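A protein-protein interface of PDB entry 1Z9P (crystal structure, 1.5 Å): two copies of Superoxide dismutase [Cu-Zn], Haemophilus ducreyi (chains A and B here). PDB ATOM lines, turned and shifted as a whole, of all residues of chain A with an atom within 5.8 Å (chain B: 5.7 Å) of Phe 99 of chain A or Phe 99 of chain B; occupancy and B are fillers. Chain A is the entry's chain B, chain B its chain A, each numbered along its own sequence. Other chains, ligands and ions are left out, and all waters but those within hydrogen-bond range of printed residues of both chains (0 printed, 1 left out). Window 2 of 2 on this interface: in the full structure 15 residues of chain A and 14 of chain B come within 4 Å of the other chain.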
ATOM      1  N   HIS A  42     -11.764 -33.433  -7.913  1.00  0.00           N
ATOM      2  CA  HIS A  42     -12.244 -32.769  -9.129  1.00  0.00           C
ATOM      3  C   HIS A  42     -11.705 -31.342  -9.242  1.00  0.00           C
ATOM      4  O   HIS A  42     -11.503 -30.674  -8.230  1.00  0.00           O
ATOM      5  CB  HIS A  42     -13.775 -32.742  -9.169  1.00  0.00           C
ATOM      6  CG  HIS A  42     -14.328 -31.768 -10.160  1.00  0.00           C
ATOM      7  ND1 HIS A  42     -14.284 -31.989 -11.520  1.00  0.00           N
ATOM      8  CD2 HIS A  42     -14.879 -30.541  -9.998  1.00  0.00           C
ATOM      9  CE1 HIS A  42     -14.808 -30.956 -12.154  1.00  0.00           C
ATOM     10  NE2 HIS A  42     -15.180 -30.063 -11.254  1.00  0.00           N
ATOM     11  N   GLY A  43     -11.466 -30.899 -10.480  1.00  0.00           N
ATOM     12  CA  GLY A  43     -11.066 -29.538 -10.771  1.00  0.00           C
ATOM     13  C   GLY A  43      -9.765 -29.470 -11.520  1.00  0.00           C
ATOM     14  O   GLY A  43      -9.240 -30.473 -11.958  1.00  0.00           O
ATOM     15  N   LEU A  44      -9.250 -28.254 -11.636  1.00  0.00           N
ATOM     16  CA  LEU A  44      -8.038 -28.005 -12.416  1.00  0.00           C
ATOM     17  C   LEU A  44      -6.864 -27.828 -11.486  1.00  0.00           C
ATOM     18  O   LEU A  44      -6.939 -27.094 -10.492  1.00  0.00           O
ATOM     19  CB  LEU A  44      -8.285 -26.761 -13.269  1.00  0.00           C
ATOM     20  CG  LEU A  44      -7.314 -26.507 -14.394  1.00  0.00           C
ATOM     21  CD1 LEU A  44      -7.478 -27.436 -15.528  1.00  0.00           C
ATOM     22  CD2 LEU A  44      -7.570 -25.034 -14.808  1.00  0.00           C
ATOM     23  N   HIS A  45      -5.815 -28.614 -11.732  1.00  0.00           N
ATOM     24  CA  HIS A  45      -4.701 -28.731 -10.822  1.00  0.00           C
ATOM     25  C   HIS A  45      -3.346 -28.295 -11.406  1.00  0.00           C
ATOM     26  O   HIS A  45      -3.058 -28.695 -12.537  1.00  0.00           O
ATOM     27  CB  HIS A  45      -4.566 -30.174 -10.334  1.00  0.00           C
ATOM     28  CG  HIS A  45      -5.743 -30.646  -9.575  1.00  0.00           C
ATOM     29  ND1 HIS A  45      -5.841 -30.499  -8.209  1.00  0.00           N
ATOM     30  CD2 HIS A  45      -6.873 -31.264  -9.981  1.00  0.00           C
ATOM     31  CE1 HIS A  45      -6.998 -31.007  -7.811  1.00  0.00           C
ATOM     32  NE2 HIS A  45      -7.630 -31.492  -8.858  1.00  0.00           N
ATOM     33  N   ALA A  97      -2.124 -26.970 -16.890  1.00  0.00           N
ATOM     34  CA  ALA A  97      -2.820 -27.569 -15.741  1.00  0.00           C
ATOM     35  C   ALA A  97      -3.649 -28.783 -16.107  1.00  0.00           C
ATOM     36  O   ALA A  97      -4.096 -28.921 -17.237  1.00  0.00           O
ATOM     37  CB  ALA A  97      -3.713 -26.498 -15.095  1.00  0.00           C
ATOM     38  N   LEU A  98      -3.800 -29.680 -15.111  1.00  0.00           N
ATOM     39  CA  LEU A  98      -4.400 -30.992 -15.277  1.00  0.00           C
ATOM     40  C   LEU A  98      -5.843 -31.010 -14.828  1.00  0.00           C
ATOM     41  O   LEU A  98      -6.144 -30.577 -13.715  1.00  0.00           O
ATOM     42  CB  LEU A  98      -3.627 -31.989 -14.442  1.00  0.00           C
ATOM     43  CG  LEU A  98      -4.184 -33.405 -14.507  1.00  0.00           C
ATOM     44  CD1 LEU A  98      -3.260 -34.267 -15.273  1.00  0.00           C
ATOM     45  CD2 LEU A  98      -4.382 -33.956 -13.109  1.00  0.00           C
ATOM     46  N   PHE A  99      -6.747 -31.443 -15.698  1.00  0.00           N
ATOM     47  CA  PHE A  99      -8.169 -31.472 -15.354  1.00  0.00           C
ATOM     48  C   PHE A  99      -8.650 -32.833 -14.857  1.00  0.00           C
ATOM     49  O   PHE A  99      -8.489 -33.827 -15.530  1.00  0.00           O
ATOM     50  CB  PHE A  99      -9.007 -31.084 -16.574  1.00  0.00           C
ATOM     51  CG  PHE A  99     -10.485 -31.152 -16.332  1.00  0.00           C
ATOM     52  CD1 PHE A  99     -11.049 -30.359 -15.373  1.00  0.00           C
ATOM     53  CD2 PHE A  99     -11.282 -32.019 -17.060  1.00  0.00           C
ATOM     54  CE1 PHE A  99     -12.405 -30.415 -15.150  1.00  0.00           C
ATOM     55  CE2 PHE A  99     -12.659 -32.076 -16.815  1.00  0.00           C
ATOM     56  CZ  PHE A  99     -13.182 -31.276 -15.889  1.00  0.00           C
ATOM     57  N   VAL A 100      -9.250 -32.812 -13.670  1.00  0.00           N
ATOM     58  CA  VAL A 100      -9.891 -33.995 -13.075  1.00  0.00           C
ATOM     59  C   VAL A 100     -11.403 -33.809 -13.126  1.00  0.00           C
ATOM     60  O   VAL A 100     -11.929 -32.816 -12.628  1.00  0.00           O
ATOM     61  CB  VAL A 100      -9.424 -34.144 -11.607  1.00  0.00           C
ATOM     62  CG1 VAL A 100     -10.087 -35.355 -10.945  1.00  0.00           C
ATOM     63  CG2 VAL A 100      -7.913 -34.302 -11.532  1.00  0.00           C
ATOM     64  N   MET A 101     -12.074 -34.753 -13.739  1.00  0.00           N
ATOM     65  CA  MET A 101     -13.542 -34.718 -13.845  1.00  0.00           C
ATOM     66  C   MET A 101     -14.212 -35.041 -12.493  1.00  0.00           C
ATOM     67  O   MET A 101     -13.557 -35.392 -11.526  1.00  0.00           O
ATOM     68  CB  MET A 101     -13.974 -35.715 -14.889  1.00  0.00           C
ATOM     69  CG  MET A 101     -13.415 -35.431 -16.271  1.00  0.00           C
ATOM     70  SD  MET A 101     -14.186 -36.372 -17.586  1.00  0.00           S
ATOM     71  CE  MET A 101     -15.726 -35.466 -17.737  1.00  0.00           C
ATOM     72  N   HIS A 102     -15.523 -34.843 -12.450  1.00  0.00           N
ATOM     73  CA  HIS A 102     -16.291 -35.058 -11.243  1.00  0.00           C
ATOM     74  C   HIS A 102     -16.176 -36.461 -10.679  1.00  0.00           C
ATOM     75  O   HIS A 102     -16.174 -36.603  -9.450  1.00  0.00           O
ATOM     76  CB  HIS A 102     -17.740 -34.716 -11.512  1.00  0.00           C
ATOM     77  CG  HIS A 102     -18.010 -33.251 -11.472  1.00  0.00           C
ATOM     78  ND1 HIS A 102     -18.443 -32.544 -12.573  1.00  0.00           N
ATOM     79  CD2 HIS A 102     -17.881 -32.349 -10.470  1.00  0.00           C
ATOM     80  CE1 HIS A 102     -18.593 -31.273 -12.247  1.00  0.00           C
ATOM     81  NE2 HIS A 102     -18.261 -31.127 -10.976  1.00  0.00           N
ATOM     82  N   SER A 105     -11.570 -38.904 -12.340  1.00  0.00           N
ATOM     83  CA  SER A 105     -10.669 -39.372 -13.384  1.00  0.00           C
ATOM     84  C   SER A 105      -9.969 -38.194 -14.036  1.00  0.00           C
ATOM     85  O   SER A 105     -10.526 -37.105 -14.129  1.00  0.00           O
ATOM     86  CB  SER A 105     -11.377 -40.194 -14.472  1.00  0.00           C
ATOM     87  OG  SER A 105     -12.336 -39.436 -15.208  1.00  0.00           O
ATOM     88  N   ALA A 106      -8.747 -38.433 -14.466  1.00  0.00           N
ATOM     89  CA  ALA A 106      -8.010 -37.449 -15.281  1.00  0.00           C
ATOM     90  C   ALA A 106      -7.527 -38.202 -16.504  1.00  0.00           C
ATOM     91  O   ALA A 106      -6.730 -39.150 -16.383  1.00  0.00           O
ATOM     92  CB  ALA A 106      -6.866 -36.875 -14.486  1.00  0.00           C
ATOM     93  N   THR A 107      -8.026 -37.798 -17.688  1.00  0.00           N
ATOM     94  CA  THR A 107      -7.688 -38.466 -18.946  1.00  0.00           C
ATOM     95  C   THR A 107      -7.488 -37.439 -20.085  1.00  0.00           C
ATOM     96  O   THR A 107      -7.411 -37.838 -21.248  1.00  0.00           O
ATOM     97  CB  THR A 107      -8.801 -39.426 -19.368  1.00  0.00           C
ATOM     98  OG1 THR A 107     -10.027 -38.724 -19.506  1.00  0.00           O
ATOM     99  CG2 THR A 107      -9.052 -40.480 -18.256  1.00  0.00           C
ATOM    100  N   THR A 108      -7.379 -36.171 -19.729  1.00  0.00           N
ATOM    101  CA  THR A 108      -7.206 -35.092 -20.734  1.00  0.00           C
ATOM    102  C   THR A 108      -5.713 -34.834 -20.986  1.00  0.00           C
ATOM    103  O   THR A 108      -4.993 -34.356 -20.131  1.00  0.00           O
ATOM    104  CB  THR A 108      -7.860 -33.835 -20.207  1.00  0.00           C
ATOM    105  OG1 THR A 108      -9.261 -34.070 -19.932  1.00  0.00           O
ATOM    106  CG2 THR A 108      -7.753 -32.708 -21.241  1.00  0.00           C
ATOM    107  N   HIS B  42     -20.567 -25.170 -16.478  1.00  0.00           N
ATOM    108  CA  HIS B  42     -19.352 -25.711 -15.871  1.00  0.00           C
ATOM    109  C   HIS B  42     -18.922 -26.997 -16.562  1.00  0.00           C
ATOM    110  O   HIS B  42     -19.767 -27.786 -16.986  1.00  0.00           O
ATOM    111  CB  HIS B  42     -19.645 -25.969 -14.400  1.00  0.00           C
ATOM    112  CG  HIS B  42     -18.619 -26.792 -13.694  1.00  0.00           C
ATOM    113  ND1 HIS B  42     -17.284 -26.453 -13.654  1.00  0.00           N
ATOM    114  CD2 HIS B  42     -18.742 -27.907 -12.930  1.00  0.00           C
ATOM    115  CE1 HIS B  42     -16.619 -27.343 -12.941  1.00  0.00           C
ATOM    116  NE2 HIS B  42     -17.483 -28.226 -12.472  1.00  0.00           N
ATOM    117  N   GLY B  43     -17.614 -27.217 -16.681  1.00  0.00           N
ATOM    118  CA  GLY B  43     -17.100 -28.428 -17.310  1.00  0.00           C
ATOM    119  C   GLY B  43     -16.044 -28.148 -18.380  1.00  0.00           C
ATOM    120  O   GLY B  43     -15.602 -26.993 -18.591  1.00  0.00           O
ATOM    121  N   LEU B  44     -15.623 -29.238 -19.014  1.00  0.00           N
ATOM    122  CA  LEU B  44     -14.637 -29.198 -20.099  1.00  0.00           C
ATOM    123  C   LEU B  44     -15.392 -29.326 -21.424  1.00  0.00           C
ATOM    124  O   LEU B  44     -16.192 -30.248 -21.616  1.00  0.00           O
ATOM    125  CB  LEU B  44     -13.668 -30.357 -19.934  1.00  0.00           C
ATOM    126  CG  LEU B  44     -12.422 -30.292 -20.793  1.00  0.00           C
ATOM    127  CD1 LEU B  44     -11.438 -29.162 -20.398  1.00  0.00           C
ATOM    128  CD2 LEU B  44     -11.695 -31.616 -20.853  1.00  0.00           C
ATOM    129  N   HIS B  45     -15.163 -28.366 -22.319  1.00  0.00           N
ATOM    130  CA  HIS B  45     -15.947 -28.223 -23.541  1.00  0.00           C
ATOM    131  C   HIS B  45     -15.080 -28.295 -24.805  1.00  0.00           C
ATOM    132  O   HIS B  45     -13.994 -27.690 -24.843  1.00  0.00           O
ATOM    133  CB  HIS B  45     -16.602 -26.845 -23.543  1.00  0.00           C
ATOM    134  CG  HIS B  45     -17.623 -26.678 -22.460  1.00  0.00           C
ATOM    135  ND1 HIS B  45     -18.934 -27.077 -22.595  1.00  0.00           N
ATOM    136  CD2 HIS B  45     -17.501 -26.178 -21.199  1.00  0.00           C
ATOM    137  CE1 HIS B  45     -19.585 -26.794 -21.474  1.00  0.00           C
ATOM    138  NE2 HIS B  45     -18.743 -26.254 -20.617  1.00  0.00           N
ATOM    139  N   ALA B  97      -9.395 -28.585 -25.366  1.00  0.00           N
ATOM    140  CA  ALA B  97     -10.682 -28.293 -24.773  1.00  0.00           C
ATOM    141  C   ALA B  97     -10.595 -27.189 -23.726  1.00  0.00           C
ATOM    142  O   ALA B  97      -9.594 -27.011 -23.069  1.00  0.00           O
ATOM    143  CB  ALA B  97     -11.228 -29.554 -24.160  1.00  0.00           C
ATOM    144  N   LEU B  98     -11.715 -26.495 -23.577  1.00  0.00           N
ATOM    145  CA  LEU B  98     -11.827 -25.317 -22.744  1.00  0.00           C
ATOM    146  C   LEU B  98     -12.522 -25.590 -21.426  1.00  0.00           C
ATOM    147  O   LEU B  98     -13.612 -26.147 -21.439  1.00  0.00           O
ATOM    148  CB  LEU B  98     -12.614 -24.272 -23.521  1.00  0.00           C
ATOM    149  CG  LEU B  98     -12.878 -22.898 -22.963  1.00  0.00           C
ATOM    150  CD1 LEU B  98     -12.820 -21.895 -24.107  1.00  0.00           C
ATOM    151  CD2 LEU B  98     -14.250 -22.855 -22.308  1.00  0.00           C
ATOM    152  N   PHE B  99     -11.911 -25.192 -20.313  1.00  0.00           N
ATOM    153  CA  PHE B  99     -12.474 -25.439 -18.978  1.00  0.00           C
ATOM    154  C   PHE B  99     -13.265 -24.257 -18.423  1.00  0.00           C
ATOM    155  O   PHE B  99     -12.758 -23.158 -18.320  1.00  0.00           O
ATOM    156  CB  PHE B  99     -11.349 -25.768 -18.009  1.00  0.00           C
ATOM    157  CG  PHE B  99     -11.839 -26.011 -16.589  1.00  0.00           C
ATOM    158  CD1 PHE B  99     -12.804 -26.984 -16.373  1.00  0.00           C
ATOM    159  CD2 PHE B  99     -11.377 -25.267 -15.525  1.00  0.00           C
ATOM    160  CE1 PHE B  99     -13.286 -27.231 -15.078  1.00  0.00           C
ATOM    161  CE2 PHE B  99     -11.865 -25.530 -14.245  1.00  0.00           C
ATOM    162  CZ  PHE B  99     -12.800 -26.492 -14.046  1.00  0.00           C
ATOM    163  N   VAL B 100     -14.503 -24.533 -18.052  1.00  0.00           N
ATOM    164  CA  VAL B 100     -15.339 -23.533 -17.422  1.00  0.00           C
ATOM    165  C   VAL B 100     -15.497 -23.944 -15.968  1.00  0.00           C
ATOM    166  O   VAL B 100     -15.925 -25.069 -15.708  1.00  0.00           O
ATOM    167  CB  VAL B 100     -16.690 -23.487 -18.079  1.00  0.00           C
ATOM    168  CG1 VAL B 100     -17.609 -22.525 -17.333  1.00  0.00           C
ATOM    169  CG2 VAL B 100     -16.557 -23.059 -19.531  1.00  0.00           C
ATOM    170  N   MET B 101     -15.149 -23.038 -15.062  1.00  0.00           N
ATOM    171  CA  MET B 101     -15.156 -23.278 -13.603  1.00  0.00           C
ATOM    172  C   MET B 101     -16.586 -23.317 -13.048  1.00  0.00           C
ATOM    173  O   MET B 101     -17.573 -23.081 -13.760  1.00  0.00           O
ATOM    174  CB  MET B 101     -14.340 -22.198 -12.894  1.00  0.00           C
ATOM    175  CG  MET B 101     -12.896 -22.081 -13.406  1.00  0.00           C
ATOM    176  SD  MET B 101     -11.717 -21.246 -12.313  1.00  0.00           S
ATOM    177  CE  MET B 101     -10.169 -21.481 -13.247  1.00  0.00           C
ATOM    178  N   HIS B 102     -16.681 -23.632 -11.747  1.00  0.00           N
ATOM    179  CA  HIS B 102     -17.969 -23.799 -11.066  1.00  0.00           C
ATOM    180  C   HIS B 102     -18.850 -22.577 -11.203  1.00  0.00           C
ATOM    181  O   HIS B 102     -20.068 -22.710 -11.339  1.00  0.00           O
ATOM    182  CB  HIS B 102     -17.781 -24.156  -9.570  1.00  0.00           C
ATOM    183  CG  HIS B 102     -17.795 -22.978  -8.640  1.00  0.00           C
ATOM    184  ND1 HIS B 102     -16.664 -22.525  -7.990  1.00  0.00           N
ATOM    185  CD2 HIS B 102     -18.808 -22.175  -8.228  1.00  0.00           C
ATOM    186  CE1 HIS B 102     -16.973 -21.480  -7.243  1.00  0.00           C
ATOM    187  NE2 HIS B 102     -18.268 -21.240  -7.376  1.00  0.00           N
ATOM    188  N   SER B 105     -17.268 -19.195 -15.192  1.00  0.00           N
ATOM    189  CA  SER B 105     -16.206 -18.409 -15.830  1.00  0.00           C
ATOM    190  C   SER B 105     -15.185 -19.323 -16.508  1.00  0.00           C
ATOM    191  O   SER B 105     -14.928 -20.459 -16.065  1.00  0.00           O
ATOM    192  CB  SER B 105     -15.483 -17.503 -14.831  1.00  0.00           C
ATOM    193  OG  SER B 105     -14.687 -18.250 -13.902  1.00  0.00           O
ATOM    194  N   ALA B 106     -14.574 -18.801 -17.566  1.00  0.00           N
ATOM    195  CA  ALA B 106     -13.496 -19.516 -18.242  1.00  0.00           C
ATOM    196  C   ALA B 106     -12.351 -18.547 -18.387  1.00  0.00           C
ATOM    197  O   ALA B 106     -12.518 -17.475 -19.009  1.00  0.00           O
ATOM    198  CB  ALA B 106     -13.971 -20.029 -19.585  1.00  0.00           C
ATOM    199  N   THR B 107     -11.192 -18.858 -17.825  1.00  0.00           N
ATOM    200  CA  THR B 107     -10.050 -17.993 -17.856  1.00  0.00           C
ATOM    201  C   THR B 107      -8.739 -18.774 -18.088  1.00  0.00           C
ATOM    202  O   THR B 107      -7.652 -18.203 -17.962  1.00  0.00           O
ATOM    203  CB  THR B 107      -9.917 -17.174 -16.577  1.00  0.00           C
ATOM    204  OG1 THR B 107      -9.768 -18.065 -15.473  1.00  0.00           O
ATOM    205  CG2 THR B 107     -11.148 -16.344 -16.286  1.00  0.00           C
ATOM    206  N   THR B 108      -8.848 -20.065 -18.453  1.00  0.00           N
ATOM    207  CA  THR B 108      -7.649 -20.903 -18.582  1.00  0.00           C
ATOM    208  C   THR B 108      -7.150 -20.892 -20.042  1.00  0.00           C
ATOM    209  O   THR B 108      -7.855 -21.377 -20.910  1.00  0.00           O
ATOM    210  CB  THR B 108      -8.035 -22.331 -18.222  1.00  0.00           C
ATOM    211  OG1 THR B 108      -8.455 -22.366 -16.859  1.00  0.00           O
ATOM    212  CG2 THR B 108      -6.811 -23.251 -18.299  1.00  0.00           C
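NE2 of His 42 of chain B lies within hydrogen-bond range of NE2 of His 42 of chain A, at 3.2 Å. A ring nitrogen (NE2) of His 102 of chain A lies close to a ring nitrogen (NE2) of His 42 of chain B.
A ring nitrogen (ND1) of His 42 of chain B is in hydrogen-bond range of the backbone carbonyl oxygen (O) of Val 100 of chain B (2.8 Å). O of Met 101 of chain B lies close to ND1 of His 42 of chain B, 3.4 Å away. A ring nitrogen (ND1) of His 42 of chain B is in hydrogen-bond range of the backbone NH (N) of His 102 of chain B (3.5 Å). ND1 of His 42 of chain A lies within hydrogen-bond range of O of Val 100 of chain A (2.7 Å). ND1 of His 42 of chain A lies close to O of Met 101 of chain A (3.5 Å). The backbone NH (N) of His 102 of chain A is in hydrogen-bond range of a ring nitrogen (ND1) of His 42 of chain A, 3.2 Å away.
Leu 44 of chain A touches Phe 99 of chain B (CD2 to CD2, 3.9 Å). Thr 108 of chain B touches Leu 44 of chain A. CE2 of Phe 99 of chain A touches CB of Leu 44 of chain B, at 3.7 Å. Phe 99 of chain A touches Phe 99 of chain B. OG1 of Thr 108 of chain A touches CD2 of Leu 44 of chain B (3.6 Å).
Phe 99 of chain B touches just these residues of chain A: Leu 44 and Phe 99. Printed residues of chain B within 4 Å of His 42 of chain A: His 42 (3.2 Å). Printed residues of chain A within 4 Å of Leu 44 of chain B: Phe 99 and Thr 108. Printed residues of chain B within 4 Å of His 102 of chain A: His 42 (3.3 Å). Ala 106 of chain A touches none of the printed residues of chain B. His 45 of chain A touches none of the printed residues of chain B. The nearest residue of chain B that does not touch Phe 99 of chain A is Gly 43 of chain B (4.9 Å). The nearest printed residue of chain B that does not touch His 102 of chain A is Gly 43 of chain B (6.0 Å).
Of the 14 printed residues of chain A, 5 touch a printed residue of chain B. Printed residues of chain A that touch a printed residue of chain B: His 42, Leu 44, Phe 99, His 102 and Thr 108. Hydrophobic or aromatic side chains of chain A within 4 Å of the printed part of chain B: His 42, Leu 44, Phe 99 and His 102.
His 42 of chain B touches its own counterpart, His 42 of chain A. Leu 44 of chain A touches Phe 99 of chain B, and with the chains exchanged Phe 99 of chain A touches Leu 44 of chain B. Phe 99 of chain A touches its own counterpart, Phe 99 of chain B. His 102 of chain A touches His 42 of chain B, but with the chains exchanged His 42 of chain A does not touch His 102 of chain B (6.6 Å).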
